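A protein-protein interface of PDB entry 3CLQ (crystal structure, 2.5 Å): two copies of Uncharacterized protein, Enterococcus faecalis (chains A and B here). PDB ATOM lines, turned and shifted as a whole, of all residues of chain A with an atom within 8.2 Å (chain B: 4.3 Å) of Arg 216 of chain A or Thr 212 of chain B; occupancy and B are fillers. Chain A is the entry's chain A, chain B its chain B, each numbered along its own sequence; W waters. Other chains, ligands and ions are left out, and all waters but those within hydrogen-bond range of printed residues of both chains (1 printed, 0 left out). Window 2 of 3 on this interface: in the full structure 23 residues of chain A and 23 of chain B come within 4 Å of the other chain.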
ATOM      1  N   VAL A 210     -25.352 -12.379   9.234  1.00  0.00           N
ATOM      2  CA  VAL A 210     -23.947 -12.603   9.448  1.00  0.00           C
ATOM      3  C   VAL A 210     -23.719 -13.435  10.714  1.00  0.00           C
ATOM      4  O   VAL A 210     -22.735 -14.173  10.823  1.00  0.00           O
ATOM      5  CB  VAL A 210     -23.229 -11.263   9.532  1.00  0.00           C
ATOM      6  CG1 VAL A 210     -21.757 -11.461   9.845  1.00  0.00           C
ATOM      7  CG2 VAL A 210     -23.397 -10.529   8.232  1.00  0.00           C
ATOM      8  N   THR A 212     -25.227 -15.911  11.527  1.00  0.00           N
ATOM      9  CA  THR A 212     -25.562 -17.251  11.127  1.00  0.00           C
ATOM     10  C   THR A 212     -24.317 -18.128  10.916  1.00  0.00           C
ATOM     11  O   THR A 212     -23.231 -17.623  10.732  1.00  0.00           O
ATOM     12  CB  THR A 212     -26.294 -17.099   9.811  1.00  0.00           C
ATOM     13  OG1 THR A 212     -27.705 -17.188  10.045  1.00  0.00           O
ATOM     14  CG2 THR A 212     -25.902 -18.120   8.837  1.00  0.00           C
ATOM     15  N   ASP A 213     -24.498 -19.444  10.937  1.00  0.00           N
ATOM     16  CA  ASP A 213     -23.480 -20.426  10.599  1.00  0.00           C
ATOM     17  C   ASP A 213     -23.106 -20.513   9.127  1.00  0.00           C
ATOM     18  O   ASP A 213     -22.201 -21.269   8.788  1.00  0.00           O
ATOM     19  CB  ASP A 213     -24.015 -21.816  10.913  1.00  0.00           C
ATOM     20  CG  ASP A 213     -23.803 -22.221  12.342  1.00  0.00           C
ATOM     21  OD1 ASP A 213     -24.747 -22.805  12.923  1.00  0.00           O
ATOM     22  OD2 ASP A 213     -22.696 -21.980  12.874  1.00  0.00           O
ATOM     23  N   PHE A 214     -23.815 -19.824   8.240  1.00  0.00           N
ATOM     24  CA  PHE A 214     -23.542 -19.971   6.819  1.00  0.00           C
ATOM     25  C   PHE A 214     -22.166 -19.396   6.471  1.00  0.00           C
ATOM     26  O   PHE A 214     -21.645 -18.541   7.189  1.00  0.00           O
ATOM     27  CB  PHE A 214     -24.682 -19.365   5.994  1.00  0.00           C
ATOM     28  CG  PHE A 214     -25.922 -20.235   5.962  1.00  0.00           C
ATOM     29  CD1 PHE A 214     -26.190 -21.047   4.864  1.00  0.00           C
ATOM     30  CD2 PHE A 214     -26.775 -20.294   7.054  1.00  0.00           C
ATOM     31  CE1 PHE A 214     -27.293 -21.880   4.846  1.00  0.00           C
ATOM     32  CE2 PHE A 214     -27.888 -21.135   7.059  1.00  0.00           C
ATOM     33  CZ  PHE A 214     -28.151 -21.930   5.951  1.00  0.00           C
ATOM     34  N   SER A 215     -21.539 -19.893   5.411  1.00  0.00           N
ATOM     35  CA  SER A 215     -20.201 -19.424   5.035  1.00  0.00           C
ATOM     36  C   SER A 215     -20.179 -18.016   4.404  1.00  0.00           C
ATOM     37  O   SER A 215     -21.191 -17.531   3.891  1.00  0.00           O
ATOM     38  CB  SER A 215     -19.580 -20.404   4.059  1.00  0.00           C
ATOM     39  OG  SER A 215     -20.429 -20.563   2.941  1.00  0.00           O
ATOM     40  N   ARG A 216     -19.008 -17.375   4.418  1.00  0.00           N
ATOM     41  CA  ARG A 216     -18.853 -16.084   3.758  1.00  0.00           C
ATOM     42  C   ARG A 216     -19.333 -16.157   2.315  1.00  0.00           C
ATOM     43  O   ARG A 216     -19.939 -15.214   1.821  1.00  0.00           O
ATOM     44  CB  ARG A 216     -17.405 -15.579   3.797  1.00  0.00           C
ATOM     45  CG  ARG A 216     -16.745 -15.651   5.156  1.00  0.00           C
ATOM     46  CD  ARG A 216     -17.332 -14.674   6.143  1.00  0.00           C
ATOM     47  NE  ARG A 216     -16.542 -13.453   6.214  1.00  0.00           N
ATOM     48  CZ  ARG A 216     -15.707 -13.137   7.201  1.00  0.00           C
ATOM     49  NH1 ARG A 216     -15.537 -13.949   8.231  1.00  0.00           N
ATOM     50  NH2 ARG A 216     -15.049 -11.992   7.165  1.00  0.00           N
ATOM     51  N   GLU A 217     -19.070 -17.278   1.649  1.00  0.00           N
ATOM     52  CA  GLU A 217     -19.416 -17.443   0.234  1.00  0.00           C
ATOM     53  C   GLU A 217     -20.926 -17.677  -0.043  1.00  0.00           C
ATOM     54  O   GLU A 217     -21.446 -17.299  -1.100  1.00  0.00           O
ATOM     55  CB  GLU A 217     -18.577 -18.566  -0.370  1.00  0.00           C
ATOM     56  CG  GLU A 217     -18.343 -18.461  -1.872  1.00  0.00           C
ATOM     57  CD  GLU A 217     -17.655 -19.716  -2.438  1.00  0.00           C
ATOM     58  OE1 GLU A 217     -18.369 -20.591  -2.987  1.00  0.00           O
ATOM     59  OE2 GLU A 217     -16.409 -19.844  -2.314  1.00  0.00           O
ATOM     60  N   GLN A 218     -21.624 -18.313   0.888  1.00  0.00           N
ATOM     61  CA  GLN A 218     -23.065 -18.459   0.744  1.00  0.00           C
ATOM     62  C   GLN A 218     -23.643 -17.093   1.029  1.00  0.00           C
ATOM     63  O   GLN A 218     -24.653 -16.674   0.448  1.00  0.00           O
ATOM     64  CB  GLN A 218     -23.628 -19.501   1.718  1.00  0.00           C
ATOM     65  CG  GLN A 218     -23.344 -20.950   1.298  1.00  0.00           C
ATOM     66  CD  GLN A 218     -23.777 -21.977   2.336  1.00  0.00           C
ATOM     67  OE1 GLN A 218     -23.323 -21.944   3.488  1.00  0.00           O
ATOM     68  NE2 GLN A 218     -24.653 -22.907   1.927  1.00  0.00           N
ATOM     69  N   LEU A 219     -22.958 -16.386   1.917  1.00  0.00           N
ATOM     70  CA  LEU A 219     -23.440 -15.123   2.411  1.00  0.00           C
ATOM     71  C   LEU A 219     -23.383 -14.143   1.247  1.00  0.00           C
ATOM     72  O   LEU A 219     -24.361 -13.449   0.945  1.00  0.00           O
ATOM     73  CB  LEU A 219     -22.556 -14.689   3.572  1.00  0.00           C
ATOM     74  CG  LEU A 219     -23.183 -14.350   4.933  1.00  0.00           C
ATOM     75  CD1 LEU A 219     -24.435 -15.115   5.234  1.00  0.00           C
ATOM     76  CD2 LEU A 219     -22.169 -14.545   6.036  1.00  0.00           C
ATOM     77  N   LYS A 220     -22.253 -14.142   0.544  1.00  0.00           N
ATOM     78  CA  LYS A 220     -22.083 -13.251  -0.593  1.00  0.00           C
ATOM     79  C   LYS A 220     -23.111 -13.510  -1.681  1.00  0.00           C
ATOM     80  O   LYS A 220     -23.711 -12.574  -2.220  1.00  0.00           O
ATOM     81  CB  LYS A 220     -20.692 -13.358  -1.189  1.00  0.00           C
ATOM     82  CG  LYS A 220     -20.388 -12.222  -2.153  1.00  0.00           C
ATOM     83  CD  LYS A 220     -19.096 -12.471  -2.920  1.00  0.00           C
ATOM     84  CE  LYS A 220     -19.320 -13.394  -4.119  1.00  0.00           C
ATOM     85  NZ  LYS A 220     -18.154 -13.304  -5.039  1.00  0.00           N
ATOM     86  N   GLU A 221     -23.313 -14.777  -2.017  1.00  0.00           N
ATOM     87  CA  GLU A 221     -24.213 -15.059  -3.108  1.00  0.00           C
ATOM     88  C   GLU A 221     -25.640 -14.687  -2.723  1.00  0.00           C
ATOM     89  O   GLU A 221     -26.424 -14.359  -3.587  1.00  0.00           O
ATOM     90  CB  GLU A 221     -24.068 -16.492  -3.627  1.00  0.00           C
ATOM     91  CG  GLU A 221     -25.019 -17.501  -3.077  1.00  0.00           C
ATOM     92  CD  GLU A 221     -24.625 -18.945  -3.453  1.00  0.00           C
ATOM     93  OE1 GLU A 221     -23.412 -19.295  -3.364  1.00  0.00           O
ATOM     94  OE2 GLU A 221     -25.522 -19.738  -3.829  1.00  0.00           O
ATOM     95  N   VAL A 222     -25.948 -14.675  -1.424  1.00  0.00           N
ATOM     96  CA  VAL A 222     -27.287 -14.328  -0.943  1.00  0.00           C
ATOM     97  C   VAL A 222     -27.422 -12.826  -0.900  1.00  0.00           C
ATOM     98  O   VAL A 222     -28.478 -12.289  -1.191  1.00  0.00           O
ATOM     99  CB  VAL A 222     -27.585 -14.926   0.448  1.00  0.00           C
ATOM    100  CG1 VAL A 222     -28.796 -14.298   1.069  1.00  0.00           C
ATOM    101  CG2 VAL A 222     -27.827 -16.406   0.328  1.00  0.00           C
ATOM    102  N   PHE A 223     -26.346 -12.142  -0.548  1.00  0.00           N
ATOM    103  CA  PHE A 223     -26.367 -10.690  -0.624  1.00  0.00           C
ATOM    104  C   PHE A 223     -26.566 -10.276  -2.058  1.00  0.00           C
ATOM    105  O   PHE A 223     -27.317  -9.349  -2.326  1.00  0.00           O
ATOM    106  CB  PHE A 223     -25.095 -10.050  -0.047  1.00  0.00           C
ATOM    107  CG  PHE A 223     -25.127  -9.927   1.429  1.00  0.00           C
ATOM    108  CD1 PHE A 223     -26.214  -9.307   2.048  1.00  0.00           C
ATOM    109  CD2 PHE A 223     -24.101 -10.465   2.213  1.00  0.00           C
ATOM    110  CE1 PHE A 223     -26.285  -9.194   3.439  1.00  0.00           C
ATOM    111  CE2 PHE A 223     -24.131 -10.366   3.616  1.00  0.00           C
ATOM    112  CZ  PHE A 223     -25.231  -9.733   4.235  1.00  0.00           C
ATOM    113  N   LEU B 162     -11.029  -1.722   6.969  1.00  0.00           N
ATOM    114  CA  LEU B 162     -12.117  -2.541   6.458  1.00  0.00           C
ATOM    115  C   LEU B 162     -12.608  -1.963   5.134  1.00  0.00           C
ATOM    116  O   LEU B 162     -12.758  -2.688   4.156  1.00  0.00           O
ATOM    117  CB  LEU B 162     -13.250  -2.604   7.470  1.00  0.00           C
ATOM    118  CG  LEU B 162     -14.305  -3.719   7.336  1.00  0.00           C
ATOM    119  CD1 LEU B 162     -15.459  -3.489   8.298  1.00  0.00           C
ATOM    120  CD2 LEU B 162     -14.854  -3.828   5.935  1.00  0.00           C
ATOM    121  N   ASP B 165     -10.018  -2.351   2.254  1.00  0.00           N
ATOM    122  CA  ASP B 165      -9.929  -3.735   1.831  1.00  0.00           C
ATOM    123  C   ASP B 165     -11.166  -4.138   1.007  1.00  0.00           C
ATOM    124  O   ASP B 165     -11.059  -4.762  -0.049  1.00  0.00           O
ATOM    125  CB  ASP B 165      -9.722  -4.647   3.044  1.00  0.00           C
ATOM    126  CG  ASP B 165      -8.337  -4.462   3.690  1.00  0.00           C
ATOM    127  OD1 ASP B 165      -7.943  -5.322   4.520  1.00  0.00           O
ATOM    128  OD2 ASP B 165      -7.631  -3.464   3.367  1.00  0.00           O
ATOM    129  N   ALA B 166     -12.343  -3.743   1.468  1.00  0.00           N
ATOM    130  CA  ALA B 166     -13.551  -4.048   0.735  1.00  0.00           C
ATOM    131  C   ALA B 166     -13.483  -3.531  -0.708  1.00  0.00           C
ATOM    132  O   ALA B 166     -13.899  -4.210  -1.643  1.00  0.00           O
ATOM    133  CB  ALA B 166     -14.737  -3.463   1.454  1.00  0.00           C
ATOM    134  N   TYR B 208     -18.826  -6.692  -0.512  1.00  0.00           N
ATOM    135  CA  TYR B 208     -17.378  -6.519  -0.495  1.00  0.00           C
ATOM    136  C   TYR B 208     -16.767  -6.607   0.900  1.00  0.00           C
ATOM    137  O   TYR B 208     -15.688  -7.174   1.063  1.00  0.00           O
ATOM    138  CB  TYR B 208     -16.995  -5.203  -1.178  1.00  0.00           C
ATOM    139  CG  TYR B 208     -17.630  -5.057  -2.528  1.00  0.00           C
ATOM    140  CD1 TYR B 208     -17.605  -6.098  -3.442  1.00  0.00           C
ATOM    141  CD2 TYR B 208     -18.286  -3.885  -2.883  1.00  0.00           C
ATOM    142  CE1 TYR B 208     -18.208  -5.983  -4.676  1.00  0.00           C
ATOM    143  CE2 TYR B 208     -18.893  -3.751  -4.116  1.00  0.00           C
ATOM    144  CZ  TYR B 208     -18.843  -4.803  -5.011  1.00  0.00           C
ATOM    145  OH  TYR B 208     -19.437  -4.661  -6.247  1.00  0.00           O
ATOM    146  N   MET B 209     -17.442  -6.060   1.902  1.00  0.00           N
ATOM    147  CA  MET B 209     -16.947  -6.151   3.262  1.00  0.00           C
ATOM    148  C   MET B 209     -16.897  -7.598   3.688  1.00  0.00           C
ATOM    149  O   MET B 209     -15.992  -8.021   4.383  1.00  0.00           O
ATOM    150  CB  MET B 209     -17.827  -5.387   4.244  1.00  0.00           C
ATOM    151  CG  MET B 209     -17.852  -3.878   4.073  1.00  0.00           C
ATOM    152  SD  MET B 209     -19.299  -3.106   5.156  1.00  0.00           S
ATOM    153  CE  MET B 209     -18.564  -3.368   6.908  1.00  0.00           C
ATOM    154  N   VAL B 210     -17.879  -8.368   3.275  1.00  0.00           N
ATOM    155  CA  VAL B 210     -17.897  -9.750   3.685  1.00  0.00           C
ATOM    156  C   VAL B 210     -16.719 -10.560   3.104  1.00  0.00           C
ATOM    157  O   VAL B 210     -16.336 -11.588   3.654  1.00  0.00           O
ATOM    158  CB  VAL B 210     -19.245 -10.362   3.333  1.00  0.00           C
ATOM    159  CG1 VAL B 210     -19.207 -11.864   3.429  1.00  0.00           C
ATOM    160  CG2 VAL B 210     -20.308  -9.774   4.249  1.00  0.00           C
ATOM    161  N   GLN B 211     -16.129 -10.075   2.013  1.00  0.00           N
ATOM    162  CA  GLN B 211     -15.052 -10.794   1.338  1.00  0.00           C
ATOM    163  C   GLN B 211     -13.696 -10.512   1.992  1.00  0.00           C
ATOM    164  O   GLN B 211     -12.638 -10.946   1.535  1.00  0.00           O
ATOM    165  CB  GLN B 211     -15.016 -10.408  -0.132  1.00  0.00           C
ATOM    166  CG  GLN B 211     -15.939 -11.239  -0.983  1.00  0.00           C
ATOM    167  CD  GLN B 211     -15.971 -10.770  -2.414  1.00  0.00           C
ATOM    168  OE1 GLN B 211     -16.866 -10.024  -2.805  1.00  0.00           O
ATOM    169  NE2 GLN B 211     -14.987 -11.184  -3.202  1.00  0.00           N
ATOM    170  N   THR B 212     -13.774  -9.799   3.099  1.00  0.00           N
ATOM    171  CA  THR B 212     -12.635  -9.201   3.735  1.00  0.00           C
ATOM    172  C   THR B 212     -12.153 -10.150   4.824  1.00  0.00           C
ATOM    173  O   THR B 212     -12.804 -11.161   5.104  1.00  0.00           O
ATOM    174  CB  THR B 212     -13.072  -7.858   4.306  1.00  0.00           C
ATOM    175  OG1 THR B 212     -12.135  -6.852   3.939  1.00  0.00           O
ATOM    176  CG2 THR B 212     -13.251  -7.924   5.797  1.00  0.00           C
ATOM    177  N   ASP B 213     -11.016  -9.859   5.431  1.00  0.00           N
ATOM    178  CA  ASP B 213     -10.522 -10.761   6.438  1.00  0.00           C
ATOM    179  C   ASP B 213     -10.889 -10.347   7.840  1.00  0.00           C
ATOM    180  O   ASP B 213     -10.468 -10.981   8.798  1.00  0.00           O
ATOM    181  CB  ASP B 213      -9.014 -10.993   6.286  1.00  0.00           C
ATOM    182  CG  ASP B 213      -8.696 -11.961   5.138  1.00  0.00           C
ATOM    183  OD1 ASP B 213      -7.480 -12.174   4.857  1.00  0.00           O
ATOM    184  OD2 ASP B 213      -9.676 -12.499   4.524  1.00  0.00           O
ATOM    185  N   PHE B 214     -11.684  -9.297   7.962  1.00  0.00           N
ATOM    186  CA  PHE B 214     -12.207  -8.896   9.265  1.00  0.00           C
ATOM    187  C   PHE B 214     -13.155  -9.961   9.856  1.00  0.00           C
ATOM    188  O   PHE B 214     -13.825 -10.696   9.125  1.00  0.00           O
ATOM    189  CB  PHE B 214     -12.836  -7.499   9.188  1.00  0.00           C
ATOM    190  CG  PHE B 214     -11.818  -6.393   9.031  1.00  0.00           C
ATOM    191  CD1 PHE B 214     -11.474  -5.589  10.108  1.00  0.00           C
ATOM    192  CD2 PHE B 214     -11.167  -6.193   7.823  1.00  0.00           C
ATOM    193  CE1 PHE B 214     -10.505  -4.582   9.970  1.00  0.00           C
ATOM    194  CE2 PHE B 214     -10.204  -5.199   7.680  1.00  0.00           C
ATOM    195  CZ  PHE B 214      -9.872  -4.390   8.750  1.00  0.00           C
ATOM    196  N   ARG B 216     -16.310 -11.766  11.968  1.00  0.00           N
ATOM    197  CA  ARG B 216     -17.746 -11.457  12.026  1.00  0.00           C
ATOM    198  C   ARG B 216     -18.004 -10.453  13.161  1.00  0.00           C
ATOM    199  O   ARG B 216     -18.700  -9.441  12.960  1.00  0.00           O
ATOM    200  CB  ARG B 216     -18.688 -12.680  12.208  1.00  0.00           C
ATOM    201  CG  ARG B 216     -18.254 -14.053  11.719  1.00  0.00           C
ATOM    202  CD  ARG B 216     -18.562 -14.417  10.280  1.00  0.00           C
ATOM    203  NE  ARG B 216     -19.860 -15.072  10.162  1.00  0.00           N
ATOM    204  CZ  ARG B 216     -20.193 -16.012   9.270  1.00  0.00           C
ATOM    205  NH1 ARG B 216     -19.317 -16.504   8.408  1.00  0.00           N
ATOM    206  NH2 ARG B 216     -21.428 -16.477   9.251  1.00  0.00           N
ATOM    207  N   LEU B 219     -17.542  -7.126  11.865  1.00  0.00           N
ATOM    208  CA  LEU B 219     -18.539  -6.702  10.933  1.00  0.00           C
ATOM    209  C   LEU B 219     -19.730  -6.294  11.769  1.00  0.00           C
ATOM    210  O   LEU B 219     -20.391  -5.310  11.464  1.00  0.00           O
ATOM    211  CB  LEU B 219     -18.890  -7.828   9.982  1.00  0.00           C
ATOM    212  CG  LEU B 219     -18.171  -7.864   8.628  1.00  0.00           C
ATOM    213  CD1 LEU B 219     -17.029  -6.920   8.577  1.00  0.00           C
ATOM    214  CD2 LEU B 219     -17.685  -9.267   8.330  1.00  0.00           C
HETATM  215  O   HOH W   1     -12.818 -13.689   5.198  1.00  0.00           O
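Water W1 lies within hydrogen-bond range of the backbone carbonyl oxygen of Thr 212 of chain B (2.5 Å), the guanidinium group of Arg 216 of chain A (3.4 Å) and the side-chain carboxylate of Asp 213 of chain B (3.4 Å).
Of the printed residues of chain B, Phe 214 of chain A touches Arg 216 (2.9 Å). Arg 216 of chain A touches just these residues of chain B: Val 210, Thr 212, Phe 214, Arg 216 and Leu 219. Of the printed residues of chain B, Leu 219 of chain A touches Arg 216 (3.8 Å). Of the printed residues of chain B, Phe 223 of chain A touches Val 210. Met 209 of chain B touches none of the printed residues of chain A. Printed residues of chain A within 4 Å of Val 210 of chain B: Arg 216 and Phe 223. Of chain A, only Arg 216 comes within 4 Å of Thr 212 of chain B. Asp 213 of chain B touches none of the printed residues of chain A. The nearest printed residue of chain B that does not touch Arg 216 of chain A is Asp 213 of chain B (4.5 Å).
NH2 of Arg 216 of chain A lies within hydrogen-bond range of O of Thr 212 of chain B. The guanidinium group of Arg 216 of chain A is in hydrogen-bond range of the backbone carbonyl oxygen of Val 210 of chain B. The backbone carbonyl oxygen (O) of Thr 212 of chain A sits at hydrogen-bond distance from the guanidinium group (NH2) of Arg 216 of chain B (2.6 Å). The backbone carbonyl oxygen (O) of Phe 214 of chain B sits at hydrogen-bond distance from the guanidinium group (NH2) of Arg 216 of chain A, at 2.6 Å. O of Phe 214 of chain A lies within hydrogen-bond range of NH2 of Arg 216 of chain B (2.9 Å). O of Val 210 of chain A is in hydrogen-bond range of NH2 of Arg 216 of chain B (3.1 Å).
Thr 212 of chain A touches Arg 216 of chain B, and with the chains exchanged Arg 216 of chain A touches Thr 212 of chain B. Phe 214 of chain A touches Arg 216 of chain B, and with the chains exchanged Arg 216 of chain A touches Phe 214 of chain B. Arg 216 of chain B touches its own counterpart, Arg 216 of chain A. Arg 216 of chain A touches Leu 219 of chain B, and with the chains exchanged Leu 219 of chain A touches Arg 216 of chain B. 6 positions are printed for both chains. Of the 11 pairs that touch across the chains among the printed residues, 9 have their exchanged pair printed and touching as well.
Of the 13 printed residues of chain A, 7 touch a printed residue of chain B. Hydrophobic or aromatic side chains of chain A within 4 Å of the printed part of chain B: Leu 219 and Phe 223. Of the 12 printed residues of chain B, 6 touch a printed residue of chain A. Among the printed residues, no Asp or Glu carboxylate lies within 4 Å of a Lys or Arg side-chain nitrogen of the other chain.
Among the printed residues, merely in contact across the chains: Lys 220 of chain A with Gln 211 of chain B, Arg 216 of chain A with Arg 216 of chain B, Leu 219 of chain A with Arg 216 of chain B, Phe 223 of chain A with Val 210 of chain B and Arg 216 of chain A with Leu 219 of chain B.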
